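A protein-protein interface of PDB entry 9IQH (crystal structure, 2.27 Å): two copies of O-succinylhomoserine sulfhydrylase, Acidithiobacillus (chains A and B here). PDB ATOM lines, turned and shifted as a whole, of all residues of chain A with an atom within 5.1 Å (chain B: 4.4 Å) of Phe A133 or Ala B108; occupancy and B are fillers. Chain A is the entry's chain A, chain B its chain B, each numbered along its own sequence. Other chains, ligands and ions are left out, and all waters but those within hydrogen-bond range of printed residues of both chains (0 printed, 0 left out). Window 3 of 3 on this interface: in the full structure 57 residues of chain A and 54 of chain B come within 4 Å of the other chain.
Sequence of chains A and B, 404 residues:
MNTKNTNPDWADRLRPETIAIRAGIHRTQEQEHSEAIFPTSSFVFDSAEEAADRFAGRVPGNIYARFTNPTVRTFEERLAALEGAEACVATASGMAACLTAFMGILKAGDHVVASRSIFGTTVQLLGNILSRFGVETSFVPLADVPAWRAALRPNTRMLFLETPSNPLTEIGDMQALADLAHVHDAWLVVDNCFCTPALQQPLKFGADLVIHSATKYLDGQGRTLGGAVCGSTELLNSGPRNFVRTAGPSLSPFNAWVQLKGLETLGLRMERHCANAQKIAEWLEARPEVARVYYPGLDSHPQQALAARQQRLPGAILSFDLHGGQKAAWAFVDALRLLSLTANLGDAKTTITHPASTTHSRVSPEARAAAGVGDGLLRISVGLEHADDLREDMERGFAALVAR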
ATOM      1  N   LYS A 107      20.548   2.450   4.057  1.00  0.00           N
ATOM      2  CA  LYS A 107      20.531   1.374   3.078  1.00  0.00           C
ATOM      3  C   LYS A 107      19.284   1.540   2.228  1.00  0.00           C
ATOM      4  O   LYS A 107      18.358   2.270   2.594  1.00  0.00           O
ATOM      5  CB  LYS A 107      20.544  -0.006   3.744  1.00  0.00           C
ATOM      6  CG  LYS A 107      19.372  -0.223   4.699  1.00  0.00           C
ATOM      7  CD  LYS A 107      19.375  -1.621   5.312  1.00  0.00           C
ATOM      8  CE  LYS A 107      18.327  -1.734   6.413  1.00  0.00           C
ATOM      9  NZ  LYS A 107      18.653  -0.839   7.568  1.00  0.00           N
ATOM     10  N   ALA A 108      19.269   0.848   1.090  1.00  0.00           N
ATOM     11  CA  ALA A 108      18.084   0.830   0.244  1.00  0.00           C
ATOM     12  C   ALA A 108      16.872   0.423   1.070  1.00  0.00           C
ATOM     13  O   ALA A 108      16.930  -0.534   1.846  1.00  0.00           O
ATOM     14  CB  ALA A 108      18.287  -0.137  -0.922  1.00  0.00           C
ATOM     15  N   ILE A 129      20.294  11.339  -6.628  1.00  0.00           N
ATOM     16  CA  ILE A 129      21.283  10.262  -6.652  1.00  0.00           C
ATOM     17  C   ILE A 129      20.891   9.125  -5.709  1.00  0.00           C
ATOM     18  O   ILE A 129      20.740   7.981  -6.136  1.00  0.00           O
ATOM     19  CB  ILE A 129      22.697  10.797  -6.333  1.00  0.00           C
ATOM     20  CG1 ILE A 129      23.185  11.719  -7.459  1.00  0.00           C
ATOM     21  CG2 ILE A 129      23.679   9.648  -6.123  1.00  0.00           C
ATOM     22  CD1 ILE A 129      24.578  12.278  -7.226  1.00  0.00           C
ATOM     23  N   LEU A 130      20.727   9.422  -4.415  1.00  0.00           N
ATOM     24  CA  LEU A 130      20.446   8.352  -3.458  1.00  0.00           C
ATOM     25  C   LEU A 130      19.052   7.777  -3.647  1.00  0.00           C
ATOM     26  O   LEU A 130      18.818   6.611  -3.316  1.00  0.00           O
ATOM     27  CB  LEU A 130      20.632   8.854  -2.027  1.00  0.00           C
ATOM     28  CG  LEU A 130      22.109   9.034  -1.679  1.00  0.00           C
ATOM     29  CD1 LEU A 130      22.285   9.385  -0.209  1.00  0.00           C
ATOM     30  CD2 LEU A 130      22.901   7.785  -2.045  1.00  0.00           C
ATOM     31  N   SER A 131      18.124   8.569  -4.187  1.00  0.00           N
ATOM     32  CA  SER A 131      16.796   8.054  -4.502  1.00  0.00           C
ATOM     33  C   SER A 131      16.874   6.895  -5.487  1.00  0.00           C
ATOM     34  O   SER A 131      16.099   5.937  -5.389  1.00  0.00           O
ATOM     35  CB  SER A 131      15.926   9.172  -5.068  1.00  0.00           C
ATOM     36  OG  SER A 131      16.466   9.636  -6.295  1.00  0.00           O
ATOM     37  N   ARG A 132      17.799   6.970  -6.451  1.00  0.00           N
ATOM     38  CA  ARG A 132      18.033   5.876  -7.388  1.00  0.00           C
ATOM     39  C   ARG A 132      18.672   4.664  -6.728  1.00  0.00           C
ATOM     40  O   ARG A 132      18.859   3.645  -7.399  1.00  0.00           O
ATOM     41  CB  ARG A 132      18.917   6.341  -8.550  1.00  0.00           C
ATOM     42  CG  ARG A 132      18.293   7.404  -9.440  1.00  0.00           C
ATOM     43  CD  ARG A 132      19.201   7.760 -10.620  1.00  0.00           C
ATOM     44  NE  ARG A 132      20.498   8.284 -10.199  1.00  0.00           N
ATOM     45  CZ  ARG A 132      21.645   7.624 -10.302  1.00  0.00           C
ATOM     46  NH1 ARG A 132      21.698   6.410 -10.828  1.00  0.00           N
ATOM     47  NH2 ARG A 132      22.768   8.200  -9.876  1.00  0.00           N
ATOM     48  N   PHE A 133      19.035   4.751  -5.448  1.00  0.00           N
ATOM     49  CA  PHE A 133      19.593   3.620  -4.723  1.00  0.00           C
ATOM     50  C   PHE A 133      18.758   3.284  -3.492  1.00  0.00           C
ATOM     51  O   PHE A 133      19.284   2.817  -2.482  1.00  0.00           O
ATOM     52  CB  PHE A 133      21.052   3.881  -4.354  1.00  0.00           C
ATOM     53  CG  PHE A 133      21.972   3.892  -5.542  1.00  0.00           C
ATOM     54  CD1 PHE A 133      22.542   2.715  -6.008  1.00  0.00           C
ATOM     55  CD2 PHE A 133      22.247   5.074  -6.212  1.00  0.00           C
ATOM     56  CE1 PHE A 133      23.382   2.723  -7.108  1.00  0.00           C
ATOM     57  CE2 PHE A 133      23.088   5.086  -7.316  1.00  0.00           C
ATOM     58  CZ  PHE A 133      23.655   3.916  -7.764  1.00  0.00           C
ATOM     59  N   GLY A 134      17.453   3.517  -3.571  1.00  0.00           N
ATOM     60  CA  GLY A 134      16.531   2.985  -2.590  1.00  0.00           C
ATOM     61  C   GLY A 134      16.351   3.805  -1.339  1.00  0.00           C
ATOM     62  O   GLY A 134      15.704   3.327  -0.400  1.00  0.00           O
ATOM     63  N   VAL A 135      16.893   5.018  -1.287  1.00  0.00           N
ATOM     64  CA  VAL A 135      16.715   5.900  -0.141  1.00  0.00           C
ATOM     65  C   VAL A 135      15.661   6.933  -0.504  1.00  0.00           C
ATOM     66  O   VAL A 135      15.809   7.661  -1.493  1.00  0.00           O
ATOM     67  CB  VAL A 135      18.032   6.572   0.272  1.00  0.00           C
ATOM     68  CG1 VAL A 135      17.789   7.543   1.413  1.00  0.00           C
ATOM     69  CG2 VAL A 135      19.062   5.533   0.672  1.00  0.00           C
ATOM     70  N   MET B 103      28.161   4.138  -9.197  1.00  0.00           N
ATOM     71  CA  MET B 103      26.994   4.923  -8.821  1.00  0.00           C
ATOM     72  C   MET B 103      26.581   5.895  -9.915  1.00  0.00           C
ATOM     73  O   MET B 103      25.406   6.276  -9.989  1.00  0.00           O
ATOM     74  CB  MET B 103      27.257   5.662  -7.509  1.00  0.00           C
ATOM     75  CG  MET B 103      27.386   4.714  -6.333  1.00  0.00           C
ATOM     76  SD  MET B 103      27.187   5.526  -4.750  1.00  0.00           S
ATOM     77  CE  MET B 103      25.427   5.860  -4.774  1.00  0.00           C
ATOM     78  N   LEU B 106      24.970   2.848 -12.487  1.00  0.00           N
ATOM     79  CA  LEU B 106      24.020   1.847 -12.047  1.00  0.00           C
ATOM     80  C   LEU B 106      22.888   2.491 -11.255  1.00  0.00           C
ATOM     81  O   LEU B 106      22.844   3.706 -11.042  1.00  0.00           O
ATOM     82  CB  LEU B 106      24.722   0.780 -11.210  1.00  0.00           C
ATOM     83  CG  LEU B 106      25.943   0.125 -11.854  1.00  0.00           C
ATOM     84  CD1 LEU B 106      26.642  -0.776 -10.849  1.00  0.00           C
ATOM     85  CD2 LEU B 106      25.553  -0.638 -13.117  1.00  0.00           C
ATOM     86  N   LYS B 107      21.955   1.649 -10.822  1.00  0.00           N
ATOM     87  CA  LYS B 107      20.898   2.031  -9.899  1.00  0.00           C
ATOM     88  C   LYS B 107      20.475   0.779  -9.144  1.00  0.00           C
ATOM     89  O   LYS B 107      20.907  -0.334  -9.459  1.00  0.00           O
ATOM     90  CB  LYS B 107      19.712   2.668 -10.629  1.00  0.00           C
ATOM     91  CG  LYS B 107      19.025   1.732 -11.601  1.00  0.00           C
ATOM     92  CD  LYS B 107      17.867   2.422 -12.309  1.00  0.00           C
ATOM     93  CE  LYS B 107      17.202   1.489 -13.308  1.00  0.00           C
ATOM     94  NZ  LYS B 107      18.213   0.896 -14.230  1.00  0.00           N
ATOM     95  N   ALA B 108      19.628   0.969  -8.134  1.00  0.00           N
ATOM     96  CA  ALA B 108      19.121  -0.174  -7.385  1.00  0.00           C
ATOM     97  C   ALA B 108      18.390  -1.121  -8.325  1.00  0.00           C
ATOM     98  O   ALA B 108      17.552  -0.697  -9.126  1.00  0.00           O
ATOM     99  CB  ALA B 108      18.190   0.286  -6.264  1.00  0.00           C
ATOM    100  N   GLY B 109      18.713  -2.407  -8.226  1.00  0.00           N
ATOM    101  CA  GLY B 109      18.128  -3.418  -9.078  1.00  0.00           C
ATOM    102  C   GLY B 109      19.010  -3.871 -10.219  1.00  0.00           C
ATOM    103  O   GLY B 109      18.657  -4.843 -10.902  1.00  0.00           O
ATOM    104  N   ASP B 110      20.136  -3.196 -10.452  1.00  0.00           N
ATOM    105  CA  ASP B 110      21.087  -3.602 -11.476  1.00  0.00           C
ATOM    106  C   ASP B 110      21.999  -4.703 -10.945  1.00  0.00           C
ATOM    107  O   ASP B 110      22.146  -4.896  -9.737  1.00  0.00           O
ATOM    108  CB  ASP B 110      21.932  -2.412 -11.946  1.00  0.00           C
ATOM    109  CG  ASP B 110      21.112  -1.352 -12.672  1.00  0.00           C
ATOM    110  OD1 ASP B 110      20.011  -1.676 -13.171  1.00  0.00           O
ATOM    111  OD2 ASP B 110      21.578  -0.192 -12.745  1.00  0.00           O
ATOM    112  N   PHE B 133      22.720  -1.174  -1.220  1.00  0.00           N
ATOM    113  CA  PHE B 133      21.953  -0.170  -1.948  1.00  0.00           C
ATOM    114  C   PHE B 133      21.369  -0.733  -3.237  1.00  0.00           C
ATOM    115  O   PHE B 133      21.177  -0.008  -4.213  1.00  0.00           O
ATOM    116  CB  PHE B 133      22.806   1.071  -2.211  1.00  0.00           C
ATOM    117  CG  PHE B 133      23.086   1.861  -0.964  1.00  0.00           C
ATOM    118  CD1 PHE B 133      22.168   2.788  -0.499  1.00  0.00           C
ATOM    119  CD2 PHE B 133      24.233   1.632  -0.223  1.00  0.00           C
ATOM    120  CE1 PHE B 133      22.402   3.493   0.666  1.00  0.00           C
ATOM    121  CE2 PHE B 133      24.471   2.338   0.938  1.00  0.00           C
ATOM    122  CZ  PHE B 133      23.553   3.269   1.383  1.00  0.00           C
ATOM    123  N   GLY B 134      21.068  -2.029  -3.241  1.00  0.00           N
ATOM    124  CA  GLY B 134      20.328  -2.645  -4.322  1.00  0.00           C
ATOM    125  C   GLY B 134      21.144  -3.130  -5.498  1.00  0.00           C
ATOM    126  O   GLY B 134      20.553  -3.516  -6.514  1.00  0.00           O
ATOM    127  N   VAL B 135      22.470  -3.129  -5.403  1.00  0.00           N
ATOM    128  CA  VAL B 135      23.331  -3.560  -6.498  1.00  0.00           C
ATOM    129  C   VAL B 135      23.805  -4.978  -6.210  1.00  0.00           C
ATOM    130  O   VAL B 135      24.444  -5.229  -5.184  1.00  0.00           O
ATOM    131  CB  VAL B 135      24.520  -2.607  -6.690  1.00  0.00           C
ATOM    132  CG1 VAL B 135      25.429  -3.107  -7.820  1.00  0.00           C
ATOM    133  CG2 VAL B 135      24.028  -1.188  -6.977  1.00  0.00           C
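NH2 of Arg A132 lies within hydrogen-bond range of O of Met B103, at 3.3 Å. The backbone carbonyl oxygen of Leu B106 is in hydrogen-bond range of the guanidinium group of Arg A132, 2.9 Å away. The backbone carbonyl oxygen (O) of Arg A132 is in hydrogen-bond range of the backbone NH (N) of Ala B108 (2.9 Å).
The backbone carbonyl oxygen (O) of Leu A130 sits at hydrogen-bond distance from the backbone NH (N) of Val A135 (3.2 Å). NZ of Lys B107 lies within salt-bridge range of OD1 of Asp B110, at 3.3 Å.
Lys A107 touches Phe B133. Phe B133 touches Ala A108. CB of Lys B107 touches O of Arg A132 (3.5 Å). Phe A133 touches Met B103 (CE2 to CE, 3.5 Å). Phe A133 touches Leu B106 (CZ to O, 3.4 Å). Phe A133 touches Lys B107 (CE1 to CA, 3.8 Å). Phe A133 touches Ala B108. Phe A133 touches Phe B133. Phe A133 touches Val B135. Val A135 touches Phe B133.
Phe A133 touches just these residues of chain B: Met B103 (3.5 Å), Leu B106 (3.4 Å), Lys B107 (3.8 Å), Ala B108 (3.9 Å), Phe B133 (3.5 Å) and Val B135 (3.97 Å). Ala B108 touches two residues of chain A. Printed residues of chain B within 4 Å of Arg A132: Met B103, Leu B106, Lys B107 and Ala B108. Printed residues of chain A within 4 Å of Met B103: Arg A132 and Phe A133. Printed residues of chain B within 4 Å of Val A135: Phe B133. Printed residues of chain B within 4 Å of Ala A108: Phe B133. Of the printed residues of chain B, Lys A107 touches Phe B133 (3.7 Å). Gly B134 touches none of the printed residues of chain A. Leu A130 touches none of the printed residues of chain B. The nearest printed residue of chain B that does not touch Phe A133 is Gly B134 (5.2 Å).
Of the 9 printed residues of chain A, 5 touch a printed residue of chain B. Hydrophobic or aromatic side chains of chain B that line the printed part of chain A: Met B103, Ala B108, Phe B133 and Val B135. Among the printed residues, no Asp or Glu carboxylate lies within 4 Å of a Lys or Arg side-chain nitrogen of the other chain.
Lys A107 touches Phe B133, and with the chains exchanged Phe A133 touches Lys B107. Ala A108 touches Phe B133, and with the chains exchanged Phe A133 touches Ala B108. Phe B133 touches its own counterpart, Phe A133. Phe A133 touches Val B135, and with the chains exchanged Val A135 touches Phe B133. 5 positions are printed for both chains.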
